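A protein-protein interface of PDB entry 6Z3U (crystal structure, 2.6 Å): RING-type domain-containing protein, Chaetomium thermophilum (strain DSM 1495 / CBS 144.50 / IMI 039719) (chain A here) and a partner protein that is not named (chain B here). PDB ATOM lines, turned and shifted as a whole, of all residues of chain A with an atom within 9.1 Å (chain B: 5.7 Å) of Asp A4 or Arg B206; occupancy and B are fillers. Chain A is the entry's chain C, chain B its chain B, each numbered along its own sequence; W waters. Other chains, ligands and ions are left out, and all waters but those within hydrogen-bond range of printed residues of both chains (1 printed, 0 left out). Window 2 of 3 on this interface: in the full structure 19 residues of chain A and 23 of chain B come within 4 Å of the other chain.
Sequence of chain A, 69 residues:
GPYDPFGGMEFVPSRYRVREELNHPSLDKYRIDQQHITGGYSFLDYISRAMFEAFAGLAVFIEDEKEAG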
ATOM      1  N   ASP A   4     -17.023 -30.329  11.627  1.00  0.00           N
ATOM      2  CA  ASP A   4     -16.081 -29.297  11.208  1.00  0.00           C
ATOM      3  C   ASP A   4     -15.616 -29.544   9.774  1.00  0.00           C
ATOM      4  O   ASP A   4     -14.937 -30.535   9.506  1.00  0.00           O
ATOM      5  CB  ASP A   4     -14.878 -29.265  12.151  1.00  0.00           C
ATOM      6  CG  ASP A   4     -13.913 -28.146  11.825  1.00  0.00           C
ATOM      7  OD1 ASP A   4     -14.255 -26.973  12.078  1.00  0.00           O
ATOM      8  OD2 ASP A   4     -12.812 -28.439  11.314  1.00  0.00           O
ATOM      9  N   PRO A   5     -15.974 -28.647   8.846  1.00  0.00           N
ATOM     10  CA  PRO A   5     -15.649 -28.899   7.436  1.00  0.00           C
ATOM     11  C   PRO A   5     -14.188 -28.685   7.090  1.00  0.00           C
ATOM     12  O   PRO A   5     -13.709 -29.287   6.119  1.00  0.00           O
ATOM     13  CB  PRO A   5     -16.542 -27.899   6.688  1.00  0.00           C
ATOM     14  CG  PRO A   5     -16.664 -26.756   7.636  1.00  0.00           C
ATOM     15  CD  PRO A   5     -16.669 -27.357   9.023  1.00  0.00           C
ATOM     16  N   PHE A   6     -13.466 -27.863   7.845  1.00  0.00           N
ATOM     17  CA  PHE A   6     -12.075 -27.552   7.549  1.00  0.00           C
ATOM     18  C   PHE A   6     -11.089 -28.496   8.224  1.00  0.00           C
ATOM     19  O   PHE A   6      -9.891 -28.200   8.256  1.00  0.00           O
ATOM     20  CB  PHE A   6     -11.771 -26.106   7.951  1.00  0.00           C
ATOM     21  CG  PHE A   6     -12.705 -25.100   7.337  1.00  0.00           C
ATOM     22  CD1 PHE A   6     -12.565 -24.726   6.010  1.00  0.00           C
ATOM     23  CD2 PHE A   6     -13.721 -24.529   8.085  1.00  0.00           C
ATOM     24  CE1 PHE A   6     -13.423 -23.804   5.441  1.00  0.00           C
ATOM     25  CE2 PHE A   6     -14.579 -23.605   7.521  1.00  0.00           C
ATOM     26  CZ  PHE A   6     -14.430 -23.242   6.197  1.00  0.00           C
ATOM     27  N   GLY A   7     -11.556 -29.623   8.757  1.00  0.00           N
ATOM     28  CA  GLY A   7     -10.657 -30.578   9.383  1.00  0.00           C
ATOM     29  C   GLY A   7      -9.800 -29.991  10.479  1.00  0.00           C
ATOM     30  O   GLY A   7      -8.641 -30.398  10.645  1.00  0.00           O
ATOM     31  N   GLY A   8     -10.337 -29.037  11.237  1.00  0.00           N
ATOM     32  CA  GLY A   8      -9.585 -28.421  12.307  1.00  0.00           C
ATOM     33  C   GLY A   8      -8.391 -27.609  11.865  1.00  0.00           C
ATOM     34  O   GLY A   8      -7.495 -27.356  12.674  1.00  0.00           O
ATOM     35  N   MET A   9      -8.350 -27.196  10.599  1.00  0.00           N
ATOM     36  CA  MET A   9      -7.244 -26.412  10.069  1.00  0.00           C
ATOM     37  C   MET A   9      -7.646 -24.985   9.719  1.00  0.00           C
ATOM     38  O   MET A   9      -6.821 -24.240   9.181  1.00  0.00           O
ATOM     39  CB  MET A   9      -6.662 -27.091   8.822  1.00  0.00           C
ATOM     40  CG  MET A   9      -6.217 -28.528   9.035  1.00  0.00           C
ATOM     41  SD  MET A   9      -4.669 -28.654   9.948  1.00  0.00           S
ATOM     42  CE  MET A   9      -4.651 -30.401  10.345  1.00  0.00           C
ATOM     43  N   GLU A  10      -8.885 -24.587  10.003  1.00  0.00           N
ATOM     44  CA  GLU A  10      -9.342 -23.252   9.639  1.00  0.00           C
ATOM     45  C   GLU A  10      -8.439 -22.195  10.260  1.00  0.00           C
ATOM     46  O   GLU A  10      -8.158 -22.225  11.462  1.00  0.00           O
ATOM     47  CB  GLU A  10     -10.788 -23.041  10.082  1.00  0.00           C
ATOM     48  CG  GLU A  10     -11.360 -21.692   9.666  1.00  0.00           C
ATOM     49  CD  GLU A  10     -12.797 -21.500  10.105  1.00  0.00           C
ATOM     50  OE1 GLU A  10     -13.477 -20.619   9.538  1.00  0.00           O
ATOM     51  OE2 GLU A  10     -13.248 -22.234  11.011  1.00  0.00           O
ATOM     52  N   PHE A  11      -7.974 -21.265   9.430  1.00  0.00           N
ATOM     53  CA  PHE A  11      -7.140 -20.163   9.886  1.00  0.00           C
ATOM     54  C   PHE A  11      -8.027 -18.971  10.226  1.00  0.00           C
ATOM     55  O   PHE A  11      -8.721 -18.439   9.352  1.00  0.00           O
ATOM     56  CB  PHE A  11      -6.114 -19.775   8.824  1.00  0.00           C
ATOM     57  CG  PHE A  11      -5.408 -18.482   9.115  1.00  0.00           C
ATOM     58  CD1 PHE A  11      -4.467 -18.404  10.128  1.00  0.00           C
ATOM     59  CD2 PHE A  11      -5.695 -17.342   8.384  1.00  0.00           C
ATOM     60  CE1 PHE A  11      -3.819 -17.215  10.401  1.00  0.00           C
ATOM     61  CE2 PHE A  11      -5.053 -16.150   8.653  1.00  0.00           C
ATOM     62  CZ  PHE A  11      -4.112 -16.086   9.663  1.00  0.00           C
ATOM     63  N   HIS B 151      -0.594 -30.659   6.025  1.00  0.00           N
ATOM     64  CA  HIS B 151      -2.010 -30.964   5.850  1.00  0.00           C
ATOM     65  C   HIS B 151      -2.192 -32.436   5.486  1.00  0.00           C
ATOM     66  O   HIS B 151      -1.381 -32.996   4.743  1.00  0.00           O
ATOM     67  CB  HIS B 151      -2.619 -30.089   4.761  1.00  0.00           C
ATOM     68  CG  HIS B 151      -4.115 -30.115   4.736  1.00  0.00           C
ATOM     69  ND1 HIS B 151      -4.834 -30.966   3.925  1.00  0.00           N
ATOM     70  CD2 HIS B 151      -5.028 -29.395   5.431  1.00  0.00           C
ATOM     71  CE1 HIS B 151      -6.126 -30.768   4.120  1.00  0.00           C
ATOM     72  NE2 HIS B 151      -6.271 -29.819   5.027  1.00  0.00           N
ATOM     73  N   ASN B 153      -4.155 -34.019   3.497  1.00  0.00           N
ATOM     74  CA  ASN B 153      -4.502 -34.323   2.114  1.00  0.00           C
ATOM     75  C   ASN B 153      -3.504 -33.736   1.120  1.00  0.00           C
ATOM     76  O   ASN B 153      -3.827 -33.593  -0.064  1.00  0.00           O
ATOM     77  CB  ASN B 153      -5.914 -33.822   1.813  1.00  0.00           C
ATOM     78  CG  ASN B 153      -6.953 -34.457   2.711  1.00  0.00           C
ATOM     79  OD1 ASN B 153      -7.578 -33.784   3.530  1.00  0.00           O
ATOM     80  ND2 ASN B 153      -7.141 -35.763   2.565  1.00  0.00           N
ATOM     81  N   MET B 201     -14.120 -36.559  -2.653  1.00  0.00           N
ATOM     82  CA  MET B 201     -14.254 -35.139  -2.956  1.00  0.00           C
ATOM     83  C   MET B 201     -13.990 -34.281  -1.724  1.00  0.00           C
ATOM     84  O   MET B 201     -13.433 -33.183  -1.834  1.00  0.00           O
ATOM     85  CB  MET B 201     -15.648 -34.862  -3.515  1.00  0.00           C
ATOM     86  CG  MET B 201     -15.859 -35.362  -4.934  1.00  0.00           C
ATOM     87  SD  MET B 201     -14.783 -34.547  -6.126  1.00  0.00           S
ATOM     88  CE  MET B 201     -15.299 -32.845  -5.932  1.00  0.00           C
ATOM     89  N   GLY B 202     -14.388 -34.759  -0.543  1.00  0.00           N
ATOM     90  CA  GLY B 202     -14.069 -34.035   0.677  1.00  0.00           C
ATOM     91  C   GLY B 202     -12.575 -33.881   0.884  1.00  0.00           C
ATOM     92  O   GLY B 202     -12.101 -32.825   1.309  1.00  0.00           O
ATOM     93  N   MET B 203     -11.816 -34.939   0.597  1.00  0.00           N
ATOM     94  CA  MET B 203     -10.364 -34.866   0.704  1.00  0.00           C
ATOM     95  C   MET B 203      -9.788 -33.891  -0.316  1.00  0.00           C
ATOM     96  O   MET B 203      -9.001 -33.003   0.032  1.00  0.00           O
ATOM     97  CB  MET B 203      -9.773 -36.263   0.515  1.00  0.00           C
ATOM     98  CG  MET B 203     -10.156 -37.223   1.623  1.00  0.00           C
ATOM     99  SD  MET B 203      -9.817 -38.939   1.211  1.00  0.00           S
ATOM    100  CE  MET B 203     -10.339 -39.759   2.714  1.00  0.00           C
ATOM    101  N   LEU B 204     -10.171 -34.045  -1.586  1.00  0.00           N
ATOM    102  CA  LEU B 204      -9.681 -33.150  -2.631  1.00  0.00           C
ATOM    103  C   LEU B 204     -10.016 -31.697  -2.317  1.00  0.00           C
ATOM    104  O   LEU B 204      -9.165 -30.811  -2.445  1.00  0.00           O
ATOM    105  CB  LEU B 204     -10.266 -33.561  -3.982  1.00  0.00           C
ATOM    106  CG  LEU B 204     -10.035 -32.600  -5.149  1.00  0.00           C
ATOM    107  CD1 LEU B 204      -8.559 -32.307  -5.310  1.00  0.00           C
ATOM    108  CD2 LEU B 204     -10.609 -33.169  -6.436  1.00  0.00           C
ATOM    109  N   THR B 205     -11.257 -31.433  -1.902  1.00  0.00           N
ATOM    110  CA  THR B 205     -11.658 -30.054  -1.637  1.00  0.00           C
ATOM    111  C   THR B 205     -10.839 -29.455  -0.498  1.00  0.00           C
ATOM    112  O   THR B 205     -10.444 -28.286  -0.559  1.00  0.00           O
ATOM    113  CB  THR B 205     -13.152 -29.993  -1.319  1.00  0.00           C
ATOM    114  OG1 THR B 205     -13.896 -30.574  -2.396  1.00  0.00           O
ATOM    115  CG2 THR B 205     -13.609 -28.556  -1.124  1.00  0.00           C
ATOM    116  N   ARG B 206     -10.554 -30.246   0.539  1.00  0.00           N
ATOM    117  CA  ARG B 206      -9.709 -29.742   1.615  1.00  0.00           C
ATOM    118  C   ARG B 206      -8.295 -29.461   1.115  1.00  0.00           C
ATOM    119  O   ARG B 206      -7.674 -28.470   1.518  1.00  0.00           O
ATOM    120  CB  ARG B 206      -9.672 -30.734   2.778  1.00  0.00           C
ATOM    121  CG  ARG B 206     -10.964 -30.825   3.574  1.00  0.00           C
ATOM    122  CD  ARG B 206     -10.761 -31.649   4.842  1.00  0.00           C
ATOM    123  NE  ARG B 206     -11.972 -31.732   5.655  1.00  0.00           N
ATOM    124  CZ  ARG B 206     -12.856 -32.725   5.597  1.00  0.00           C
ATOM    125  NH1 ARG B 206     -12.678 -33.744   4.763  1.00  0.00           N
ATOM    126  NH2 ARG B 206     -13.925 -32.696   6.382  1.00  0.00           N
ATOM    127  N   ALA B 207      -7.782 -30.303   0.216  1.00  0.00           N
ATOM    128  CA  ALA B 207      -6.442 -30.081  -0.315  1.00  0.00           C
ATOM    129  C   ALA B 207      -6.373 -28.773  -1.091  1.00  0.00           C
ATOM    130  O   ALA B 207      -5.488 -27.944  -0.852  1.00  0.00           O
ATOM    131  CB  ALA B 207      -6.029 -31.256  -1.201  1.00  0.00           C
ATOM    132  N   VAL B 208      -7.310 -28.562  -2.017  1.00  0.00           N
ATOM    133  CA  VAL B 208      -7.299 -27.323  -2.788  1.00  0.00           C
ATOM    134  C   VAL B 208      -7.614 -26.134  -1.892  1.00  0.00           C
ATOM    135  O   VAL B 208      -7.076 -25.039  -2.093  1.00  0.00           O
ATOM    136  CB  VAL B 208      -8.277 -27.414  -3.972  1.00  0.00           C
ATOM    137  CG1 VAL B 208      -8.293 -26.118  -4.753  1.00  0.00           C
ATOM    138  CG2 VAL B 208      -7.891 -28.560  -4.874  1.00  0.00           C
ATOM    139  N   TRP B 209      -8.479 -26.317  -0.893  1.00  0.00           N
ATOM    140  CA  TRP B 209      -8.712 -25.240   0.062  1.00  0.00           C
ATOM    141  C   TRP B 209      -7.423 -24.868   0.779  1.00  0.00           C
ATOM    142  O   TRP B 209      -7.113 -23.683   0.941  1.00  0.00           O
ATOM    143  CB  TRP B 209      -9.783 -25.648   1.073  1.00  0.00           C
ATOM    144  CG  TRP B 209      -9.875 -24.712   2.247  1.00  0.00           C
ATOM    145  CD1 TRP B 209     -10.562 -23.535   2.309  1.00  0.00           C
ATOM    146  CD2 TRP B 209      -9.247 -24.879   3.525  1.00  0.00           C
ATOM    147  NE1 TRP B 209     -10.405 -22.962   3.548  1.00  0.00           N
ATOM    148  CE2 TRP B 209      -9.602 -23.766   4.312  1.00  0.00           C
ATOM    149  CE3 TRP B 209      -8.423 -25.862   4.080  1.00  0.00           C
ATOM    150  CZ2 TRP B 209      -9.160 -23.609   5.622  1.00  0.00           C
ATOM    151  CZ3 TRP B 209      -7.985 -25.704   5.381  1.00  0.00           C
ATOM    152  CH2 TRP B 209      -8.354 -24.587   6.138  1.00  0.00           C
ATOM    153  N   TRP B 210      -6.647 -25.869   1.199  1.00  0.00           N
ATOM    154  CA  TRP B 210      -5.402 -25.592   1.905  1.00  0.00           C
ATOM    155  C   TRP B 210      -4.383 -24.922   0.993  1.00  0.00           C
ATOM    156  O   TRP B 210      -3.638 -24.035   1.429  1.00  0.00           O
ATOM    157  CB  TRP B 210      -4.838 -26.887   2.486  1.00  0.00           C
ATOM    158  CG  TRP B 210      -3.589 -26.693   3.269  1.00  0.00           C
ATOM    159  CD1 TRP B 210      -2.370 -27.237   3.006  1.00  0.00           C
ATOM    160  CD2 TRP B 210      -3.426 -25.884   4.439  1.00  0.00           C
ATOM    161  NE1 TRP B 210      -1.456 -26.827   3.946  1.00  0.00           N
ATOM    162  CE2 TRP B 210      -2.081 -25.996   4.837  1.00  0.00           C
ATOM    163  CE3 TRP B 210      -4.289 -25.079   5.190  1.00  0.00           C
ATOM    164  CZ2 TRP B 210      -1.576 -25.334   5.953  1.00  0.00           C
ATOM    165  CZ3 TRP B 210      -3.787 -24.424   6.297  1.00  0.00           C
ATOM    166  CH2 TRP B 210      -2.443 -24.555   6.667  1.00  0.00           C
ATOM    167  N   CYS B 211      -4.334 -25.330  -0.276  1.00  0.00           N
ATOM    168  CA  CYS B 211      -3.452 -24.663  -1.228  1.00  0.00           C
ATOM    169  C   CYS B 211      -3.790 -23.183  -1.324  1.00  0.00           C
ATOM    170  O   CYS B 211      -2.914 -22.321  -1.190  1.00  0.00           O
ATOM    171  CB  CYS B 211      -3.570 -25.321  -2.602  1.00  0.00           C
ATOM    172  SG  CYS B 211      -2.833 -26.960  -2.714  1.00  0.00           S
ATOM    173  N   LEU B 378     -16.416 -26.048   0.918  1.00  0.00           N
ATOM    174  CA  LEU B 378     -16.393 -26.862   2.127  1.00  0.00           C
ATOM    175  C   LEU B 378     -17.615 -26.647   3.010  1.00  0.00           C
ATOM    176  O   LEU B 378     -17.958 -27.538   3.794  1.00  0.00           O
ATOM    177  CB  LEU B 378     -15.126 -26.575   2.932  1.00  0.00           C
ATOM    178  CG  LEU B 378     -13.823 -27.111   2.338  1.00  0.00           C
ATOM    179  CD1 LEU B 378     -12.634 -26.607   3.135  1.00  0.00           C
ATOM    180  CD2 LEU B 378     -13.828 -28.638   2.295  1.00  0.00           C
HETATM  181  O   HOH W   1     -15.951 -31.145   4.845  1.00  0.00           O
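The backbone carbonyl oxygen (O) of Pro A5 is in hydrogen-bond range of the guanidinium group (NE) of Arg B206, at 3.0 Å.
Arg B206 touches Asp A4.
Leu B378 touches Pro A5 (O to CB, 3.2 Å).
Phe A6 touches Trp B209.
Leu B378 touches Phe A6.
Arg B206 touches Gly A7 (NE to N, 3.8 Å).
Met A9 touches His B151 (CG to CD2, 3.9 Å).
Met A9 touches Trp B209 (O to CH2, 3.4 Å).
Glu A10 touches Trp B209.
ND1 of His B151 is in hydrogen-bond range of N of Asn B153 (3.2 Å).
The backbone NH (N) of Gly A7 lies within hydrogen-bond range of the side-chain carboxylate (OD2) of Asp A4, 3.1 Å away.
The side-chain carboxylate (OD2) of Asp A4 sits at hydrogen-bond distance from the backbone NH (N) of Gly A8, 2.5 Å away.
Asp A4 touches just one residue of chain B: Arg B206 (3.9 Å).
Of the printed residues of chain B, Pro A5 touches Arg B206 (3.0 Å) and Leu B378 (3.2 Å).
Of the printed residues of chain B, Phe A6 touches Trp B209 and Leu B378.
Gly A8 touches none of the printed residues of chain B.
Printed residues of chain B within 4 Å of Met A9: His B151 and Trp B209.
Of chain A, only Asp A4, Pro A5 and Gly A7 come within 4 Å of Arg B206.
No residue of chain A comes within 4 Å of Ala B207.
Printed residues of chain A within 4 Å of Leu B378: Pro A5 (3.2 Å) and Phe A6 (3.4 Å).
The nearest printed residue of chain A that does not touch Leu B378 is Gly A7 (6.5 Å).
Water W1 bridges NH2 of Arg B206 (3.0 Å) and O of Pro A5 (3.2 Å).
Of the 8 printed residues of chain A, 6 touch a printed residue of chain B.
Printed residues of chain A that touch a printed residue of chain B: Asp A4, Pro A5, Phe A6, Gly A7, Met A9 and Glu A10.
Hydrophobic or aromatic side chains of chain A that line the printed part of chain B: Pro A5, Phe A6 and Met A9.
Of the 14 printed residues of chain B, 4 touch a printed residue of chain A.
Printed residues of chain B that touch a printed residue of chain A: His B151, Arg B206, Trp B209 and Leu B378.
Along chain B the printed residues that touch a printed residue of chain A span positions 151 to 378.
Among the printed residues, 9 pairs touch across the chains.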
